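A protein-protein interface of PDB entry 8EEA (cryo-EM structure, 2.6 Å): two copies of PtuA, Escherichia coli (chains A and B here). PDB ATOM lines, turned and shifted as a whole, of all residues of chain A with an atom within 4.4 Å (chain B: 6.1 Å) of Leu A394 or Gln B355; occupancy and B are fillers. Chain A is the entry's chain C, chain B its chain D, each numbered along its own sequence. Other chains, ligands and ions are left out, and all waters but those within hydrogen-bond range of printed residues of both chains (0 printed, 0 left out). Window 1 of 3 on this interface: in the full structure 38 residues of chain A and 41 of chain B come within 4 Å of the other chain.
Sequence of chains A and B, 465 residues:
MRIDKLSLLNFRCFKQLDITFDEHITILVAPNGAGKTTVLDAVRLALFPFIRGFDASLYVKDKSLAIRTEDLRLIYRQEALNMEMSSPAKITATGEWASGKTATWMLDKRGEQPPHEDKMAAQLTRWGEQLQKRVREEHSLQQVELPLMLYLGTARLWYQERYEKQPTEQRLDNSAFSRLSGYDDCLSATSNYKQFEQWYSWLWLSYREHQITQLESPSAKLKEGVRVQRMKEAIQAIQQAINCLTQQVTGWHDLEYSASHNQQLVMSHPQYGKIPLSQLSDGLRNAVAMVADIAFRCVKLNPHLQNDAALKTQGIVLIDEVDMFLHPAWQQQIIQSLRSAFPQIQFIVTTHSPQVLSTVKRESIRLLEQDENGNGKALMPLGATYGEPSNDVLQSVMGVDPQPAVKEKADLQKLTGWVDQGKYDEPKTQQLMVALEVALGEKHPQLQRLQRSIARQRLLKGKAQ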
ATOM      1  N   PRO A 354     -28.254 -25.138  -6.324  1.00  0.00           N
ATOM      2  CA  PRO A 354     -29.438 -24.495  -5.730  1.00  0.00           C
ATOM      3  C   PRO A 354     -30.629 -24.392  -6.668  1.00  0.00           C
ATOM      4  O   PRO A 354     -31.760 -24.240  -6.184  1.00  0.00           O
ATOM      5  CB  PRO A 354     -28.924 -23.103  -5.342  1.00  0.00           C
ATOM      6  CG  PRO A 354     -27.801 -22.841  -6.264  1.00  0.00           C
ATOM      7  CD  PRO A 354     -27.192 -24.163  -6.631  1.00  0.00           C
ATOM      8  N   SER A 390     -32.815 -18.348  -6.706  1.00  0.00           N
ATOM      9  CA  SER A 390     -31.624 -19.169  -6.522  1.00  0.00           C
ATOM     10  C   SER A 390     -30.634 -18.517  -5.565  1.00  0.00           C
ATOM     11  O   SER A 390     -29.993 -19.207  -4.765  1.00  0.00           O
ATOM     12  CB  SER A 390     -30.957 -19.440  -7.870  1.00  0.00           C
ATOM     13  OG  SER A 390     -31.732 -20.327  -8.654  1.00  0.00           O
ATOM     14  N   ASN A 391     -30.476 -17.194  -5.643  1.00  0.00           N
ATOM     15  CA  ASN A 391     -29.522 -16.524  -4.762  1.00  0.00           C
ATOM     16  C   ASN A 391     -29.938 -16.640  -3.301  1.00  0.00           C
ATOM     17  O   ASN A 391     -29.088 -16.801  -2.417  1.00  0.00           O
ATOM     18  CB  ASN A 391     -29.363 -15.057  -5.163  1.00  0.00           C
ATOM     19  CG  ASN A 391     -30.687 -14.339  -5.294  1.00  0.00           C
ATOM     20  OD1 ASN A 391     -31.719 -14.957  -5.547  1.00  0.00           O
ATOM     21  ND2 ASN A 391     -30.668 -13.024  -5.111  1.00  0.00           N
ATOM     22  N   ASP A 392     -31.242 -16.561  -3.021  1.00  0.00           N
ATOM     23  CA  ASP A 392     -31.708 -16.713  -1.646  1.00  0.00           C
ATOM     24  C   ASP A 392     -31.430 -18.116  -1.116  1.00  0.00           C
ATOM     25  O   ASP A 392     -30.996 -18.276   0.031  1.00  0.00           O
ATOM     26  CB  ASP A 392     -33.198 -16.390  -1.560  1.00  0.00           C
ATOM     27  CG  ASP A 392     -33.497 -14.938  -1.875  1.00  0.00           C
ATOM     28  OD1 ASP A 392     -33.476 -14.108  -0.941  1.00  0.00           O
ATOM     29  OD2 ASP A 392     -33.752 -14.623  -3.054  1.00  0.00           O
ATOM     30  N   VAL A 393     -31.672 -19.143  -1.933  1.00  0.00           N
ATOM     31  CA  VAL A 393     -31.378 -20.509  -1.515  1.00  0.00           C
ATOM     32  C   VAL A 393     -29.879 -20.693  -1.315  1.00  0.00           C
ATOM     33  O   VAL A 393     -29.441 -21.369  -0.377  1.00  0.00           O
ATOM     34  CB  VAL A 393     -31.937 -21.511  -2.543  1.00  0.00           C
ATOM     35  CG1 VAL A 393     -31.525 -22.928  -2.185  1.00  0.00           C
ATOM     36  CG2 VAL A 393     -33.448 -21.397  -2.620  1.00  0.00           C
ATOM     37  N   LEU A 394     -29.073 -20.101  -2.196  1.00  0.00           N
ATOM     38  CA  LEU A 394     -27.625 -20.181  -2.055  1.00  0.00           C
ATOM     39  C   LEU A 394     -27.166 -19.556  -0.745  1.00  0.00           C
ATOM     40  O   LEU A 394     -26.307 -20.110  -0.051  1.00  0.00           O
ATOM     41  CB  LEU A 394     -26.958 -19.489  -3.244  1.00  0.00           C
ATOM     42  CG  LEU A 394     -25.470 -19.738  -3.476  1.00  0.00           C
ATOM     43  CD1 LEU A 394     -25.227 -21.116  -4.050  1.00  0.00           C
ATOM     44  CD2 LEU A 394     -24.910 -18.670  -4.401  1.00  0.00           C
ATOM     45  N   GLN A 395     -27.727 -18.401  -0.389  1.00  0.00           N
ATOM     46  CA  GLN A 395     -27.301 -17.721   0.830  1.00  0.00           C
ATOM     47  C   GLN A 395     -27.792 -18.448   2.075  1.00  0.00           C
ATOM     48  O   GLN A 395     -27.066 -18.538   3.072  1.00  0.00           O
ATOM     49  CB  GLN A 395     -27.799 -16.275   0.820  1.00  0.00           C
ATOM     50  CG  GLN A 395     -27.421 -15.467   2.056  1.00  0.00           C
ATOM     51  CD  GLN A 395     -26.000 -14.951   2.003  1.00  0.00           C
ATOM     52  OE1 GLN A 395     -25.683 -14.049   1.228  1.00  0.00           O
ATOM     53  NE2 GLN A 395     -25.131 -15.524   2.828  1.00  0.00           N
ATOM     54  N   SER A 396     -29.017 -18.973   2.044  1.00  0.00           N
ATOM     55  CA  SER A 396     -29.633 -19.534   3.244  1.00  0.00           C
ATOM     56  C   SER A 396     -29.286 -21.010   3.434  1.00  0.00           C
ATOM     57  O   SER A 396     -28.731 -21.395   4.467  1.00  0.00           O
ATOM     58  CB  SER A 396     -31.151 -19.347   3.181  1.00  0.00           C
ATOM     59  OG  SER A 396     -31.755 -19.684   4.419  1.00  0.00           O
ATOM     60  N   MET A 398     -27.162 -23.056   1.695  1.00  0.00           N
ATOM     61  CA  MET A 398     -25.764 -23.428   1.524  1.00  0.00           C
ATOM     62  C   MET A 398     -24.793 -22.500   2.239  1.00  0.00           C
ATOM     63  O   MET A 398     -23.644 -22.894   2.463  1.00  0.00           O
ATOM     64  CB  MET A 398     -25.414 -23.463   0.032  1.00  0.00           C
ATOM     65  CG  MET A 398     -26.197 -24.503  -0.744  1.00  0.00           C
ATOM     66  SD  MET A 398     -25.799 -24.541  -2.497  1.00  0.00           S
ATOM     67  CE  MET A 398     -26.946 -25.794  -3.055  1.00  0.00           C
ATOM     68  N   GLY A 399     -25.217 -21.294   2.601  1.00  0.00           N
ATOM     69  CA  GLY A 399     -24.335 -20.380   3.300  1.00  0.00           C
ATOM     70  C   GLY A 399     -23.275 -19.737   2.439  1.00  0.00           C
ATOM     71  O   GLY A 399     -22.250 -19.298   2.965  1.00  0.00           O
ATOM     72  N   VAL A 400     -23.490 -19.661   1.128  1.00  0.00           N
ATOM     73  CA  VAL A 400     -22.532 -19.088   0.190  1.00  0.00           C
ATOM     74  C   VAL A 400     -23.066 -17.742  -0.277  1.00  0.00           C
ATOM     75  O   VAL A 400     -24.220 -17.639  -0.708  1.00  0.00           O
ATOM     76  CB  VAL A 400     -22.285 -20.027  -1.003  1.00  0.00           C
ATOM     77  CG1 VAL A 400     -21.214 -19.459  -1.919  1.00  0.00           C
ATOM     78  CG2 VAL A 400     -21.894 -21.410  -0.515  1.00  0.00           C
ATOM     79  N   PRO A 402     -23.846 -14.914  -2.729  1.00  0.00           N
ATOM     80  CA  PRO A 402     -23.941 -14.880  -4.199  1.00  0.00           C
ATOM     81  C   PRO A 402     -22.939 -13.947  -4.857  1.00  0.00           C
ATOM     82  O   PRO A 402     -22.764 -14.020  -6.079  1.00  0.00           O
ATOM     83  CB  PRO A 402     -25.384 -14.418  -4.451  1.00  0.00           C
ATOM     84  CG  PRO A 402     -25.846 -13.827  -3.170  1.00  0.00           C
ATOM     85  CD  PRO A 402     -25.119 -14.547  -2.090  1.00  0.00           C
ATOM     86  N   PRO B 328     -20.598 -24.945  -5.225  1.00  0.00           N
ATOM     87  CA  PRO B 328     -20.559 -23.517  -5.590  1.00  0.00           C
ATOM     88  C   PRO B 328     -19.463 -22.717  -4.908  1.00  0.00           C
ATOM     89  O   PRO B 328     -18.930 -21.784  -5.520  1.00  0.00           O
ATOM     90  CB  PRO B 328     -21.952 -23.019  -5.182  1.00  0.00           C
ATOM     91  CG  PRO B 328     -22.813 -24.218  -5.243  1.00  0.00           C
ATOM     92  CD  PRO B 328     -21.951 -25.370  -4.827  1.00  0.00           C
ATOM     93  N   ALA B 329     -19.115 -23.028  -3.658  1.00  0.00           N
ATOM     94  CA  ALA B 329     -18.031 -22.301  -3.007  1.00  0.00           C
ATOM     95  C   ALA B 329     -16.695 -22.583  -3.684  1.00  0.00           C
ATOM     96  O   ALA B 329     -15.838 -21.697  -3.771  1.00  0.00           O
ATOM     97  CB  ALA B 329     -17.967 -22.664  -1.524  1.00  0.00           C
ATOM     98  N   GLN B 331     -16.482 -23.380  -6.889  1.00  0.00           N
ATOM     99  CA  GLN B 331     -16.580 -22.833  -8.235  1.00  0.00           C
ATOM    100  C   GLN B 331     -16.173 -21.367  -8.299  1.00  0.00           C
ATOM    101  O   GLN B 331     -15.839 -20.879  -9.382  1.00  0.00           O
ATOM    102  CB  GLN B 331     -18.004 -22.991  -8.761  1.00  0.00           C
ATOM    103  CG  GLN B 331     -18.387 -24.420  -9.096  1.00  0.00           C
ATOM    104  CD  GLN B 331     -19.870 -24.579  -9.349  1.00  0.00           C
ATOM    105  OE1 GLN B 331     -20.567 -23.612  -9.642  1.00  0.00           O
ATOM    106  NE2 GLN B 331     -20.360 -25.805  -9.239  1.00  0.00           N
ATOM    107  N   GLN B 332     -16.186 -20.662  -7.174  1.00  0.00           N
ATOM    108  CA  GLN B 332     -15.844 -19.248  -7.130  1.00  0.00           C
ATOM    109  C   GLN B 332     -14.350 -19.006  -6.965  1.00  0.00           C
ATOM    110  O   GLN B 332     -13.938 -17.854  -6.815  1.00  0.00           O
ATOM    111  CB  GLN B 332     -16.599 -18.565  -5.987  1.00  0.00           C
ATOM    112  CG  GLN B 332     -18.098 -18.497  -6.192  1.00  0.00           C
ATOM    113  CD  GLN B 332     -18.801 -17.739  -5.090  1.00  0.00           C
ATOM    114  OE1 GLN B 332     -18.327 -17.690  -3.956  1.00  0.00           O
ATOM    115  NE2 GLN B 332     -19.941 -17.146  -5.414  1.00  0.00           N
ATOM    116  N   SER B 353     -21.651 -22.503 -15.472  1.00  0.00           N
ATOM    117  CA  SER B 353     -21.932 -22.177 -14.082  1.00  0.00           C
ATOM    118  C   SER B 353     -21.831 -20.674 -13.878  1.00  0.00           C
ATOM    119  O   SER B 353     -20.771 -20.097 -14.165  1.00  0.00           O
ATOM    120  CB  SER B 353     -20.956 -22.906 -13.161  1.00  0.00           C
ATOM    121  OG  SER B 353     -21.174 -22.555 -11.807  1.00  0.00           O
ATOM    122  N   PRO B 354     -22.876 -19.992 -13.400  1.00  0.00           N
ATOM    123  CA  PRO B 354     -22.743 -18.546 -13.154  1.00  0.00           C
ATOM    124  C   PRO B 354     -21.680 -18.201 -12.129  1.00  0.00           C
ATOM    125  O   PRO B 354     -21.096 -17.111 -12.194  1.00  0.00           O
ATOM    126  CB  PRO B 354     -24.145 -18.140 -12.674  1.00  0.00           C
ATOM    127  CG  PRO B 354     -24.795 -19.405 -12.242  1.00  0.00           C
ATOM    128  CD  PRO B 354     -24.238 -20.473 -13.115  1.00  0.00           C
ATOM    129  N   GLN B 355     -21.408 -19.097 -11.178  1.00  0.00           N
ATOM    130  CA  GLN B 355     -20.400 -18.816 -10.164  1.00  0.00           C
ATOM    131  C   GLN B 355     -19.023 -18.639 -10.788  1.00  0.00           C
ATOM    132  O   GLN B 355     -18.244 -17.780 -10.360  1.00  0.00           O
ATOM    133  CB  GLN B 355     -20.377 -19.937  -9.126  1.00  0.00           C
ATOM    134  CG  GLN B 355     -21.419 -19.790  -8.029  1.00  0.00           C
ATOM    135  CD  GLN B 355     -22.733 -20.452  -8.384  1.00  0.00           C
ATOM    136  OE1 GLN B 355     -22.760 -21.549  -8.937  1.00  0.00           O
ATOM    137  NE2 GLN B 355     -23.834 -19.786  -8.062  1.00  0.00           N
ATOM    138  N   VAL B 356     -18.696 -19.454 -11.793  1.00  0.00           N
ATOM    139  CA  VAL B 356     -17.422 -19.295 -12.487  1.00  0.00           C
ATOM    140  C   VAL B 356     -17.427 -18.023 -13.326  1.00  0.00           C
ATOM    141  O   VAL B 356     -16.424 -17.303 -13.392  1.00  0.00           O
ATOM    142  CB  VAL B 356     -17.129 -20.536 -13.350  1.00  0.00           C
ATOM    143  CG1 VAL B 356     -15.762 -20.420 -14.000  1.00  0.00           C
ATOM    144  CG2 VAL B 356     -17.213 -21.797 -12.515  1.00  0.00           C
ATOM    145  N   LEU B 357     -18.551 -17.725 -13.980  1.00  0.00           N
ATOM    146  CA  LEU B 357     -18.604 -16.578 -14.880  1.00  0.00           C
ATOM    147  C   LEU B 357     -18.572 -15.257 -14.126  1.00  0.00           C
ATOM    148  O   LEU B 357     -18.248 -14.219 -14.713  1.00  0.00           O
ATOM    149  CB  LEU B 357     -19.857 -16.654 -15.748  1.00  0.00           C
ATOM    150  CG  LEU B 357     -19.865 -17.728 -16.834  1.00  0.00           C
ATOM    151  CD1 LEU B 357     -21.201 -17.743 -17.553  1.00  0.00           C
ATOM    152  CD2 LEU B 357     -18.731 -17.516 -17.820  1.00  0.00           C
ATOM    153  N   SER B 358     -18.903 -15.266 -12.834  1.00  0.00           N
ATOM    154  CA  SER B 358     -18.889 -14.025 -12.070  1.00  0.00           C
ATOM    155  C   SER B 358     -17.498 -13.640 -11.590  1.00  0.00           C
ATOM    156  O   SER B 358     -17.359 -12.614 -10.915  1.00  0.00           O
ATOM    157  CB  SER B 358     -19.828 -14.138 -10.868  1.00  0.00           C
ATOM    158  OG  SER B 358     -19.625 -15.357 -10.178  1.00  0.00           O
ATOM    159  N   THR B 359     -16.472 -14.423 -11.918  1.00  0.00           N
ATOM    160  CA  THR B 359     -15.120 -14.194 -11.429  1.00  0.00           C
ATOM    161  C   THR B 359     -14.144 -13.793 -12.530  1.00  0.00           C
ATOM    162  O   THR B 359     -12.941 -13.708 -12.272  1.00  0.00           O
ATOM    163  CB  THR B 359     -14.606 -15.447 -10.717  1.00  0.00           C
ATOM    164  OG1 THR B 359     -14.634 -16.559 -11.620  1.00  0.00           O
ATOM    165  CG2 THR B 359     -15.464 -15.761  -9.502  1.00  0.00           C
ATOM    166  N   SER B 390     -24.546 -13.720  -8.641  1.00  0.00           N
ATOM    167  CA  SER B 390     -24.733 -14.873  -9.516  1.00  0.00           C
ATOM    168  C   SER B 390     -26.024 -14.771 -10.320  1.00  0.00           C
ATOM    169  O   SER B 390     -26.055 -15.154 -11.493  1.00  0.00           O
ATOM    170  CB  SER B 390     -24.718 -16.158  -8.692  1.00  0.00           C
ATOM    171  OG  SER B 390     -23.424 -16.411  -8.180  1.00  0.00           O
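2 positions are printed for both chains. Of the 4 pairs that touch across the chains among the printed residues, none has its exchanged pair printed and touching as well.
The side-chain hydroxyl (OG) of Ser B353 lies within hydrogen-bond range of the side-chain amide oxygen (OE1) of Gln B355 (3.4 Å). O of Gln B355 is in hydrogen-bond range of OG of Ser B358. OE1 of Gln B331 sits close to OE1 of Gln B355 (3.1 Å). The backbone carbonyl oxygen (O) of Leu A394 lies within hydrogen-bond range of the backbone NH (N) of Gly A399. NE2 of Gln B355 lies within hydrogen-bond range of OG of Ser B390 (3.4 Å). The backbone carbonyl oxygen (O) of Leu A394 sits at hydrogen-bond distance from the backbone NH (N) of Val A400 (3.1 Å).
Of the 12 printed residues of chain B, 4 touch a printed residue of chain A. Hydrophobic or aromatic side chains of chain B that line the printed part of chain A: Pro B328. Of the 12 printed residues of chain A, 3 touch a printed residue of chain B. Printed residues of chain A that touch a printed residue of chain B: Leu A394, Val A400 and Pro A402. Hydrophobic or aromatic side chains of chain A that line the printed part of chain B: Leu A394 and Val A400. Among the printed residues, 4 pairs touch across the chains.
Among the printed residues, pairs that only touch across the chains: Leu A394 with Pro B328 (3.95 Å), Leu A394 with Gln B355 (3.98 Å) and Val A400 with Gln B332 (3.95 Å).
The backbone carbonyl oxygen (O) of Pro A402 is in hydrogen-bond range of the backbone NH (N) of Ser B390 (3.1 Å).
Leu A394 touches just these residues of chain B: Pro B328 (3.95 Å) and Gln B355 (3.98 Å). Printed residues of chain B within 4 Å of Pro A402: Ser B390. Printed residues of chain A within 4 Å of Pro B328: Leu A394. Of the printed residues of chain A, Gln B332 touches Val A400. Ser B353 touches none of the printed residues of chain A. Printed residues of chain A within 4 Å of Gln B355: Leu A394. Of the printed residues of chain A, Ser B390 touches Pro A402 (3.1 Å).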
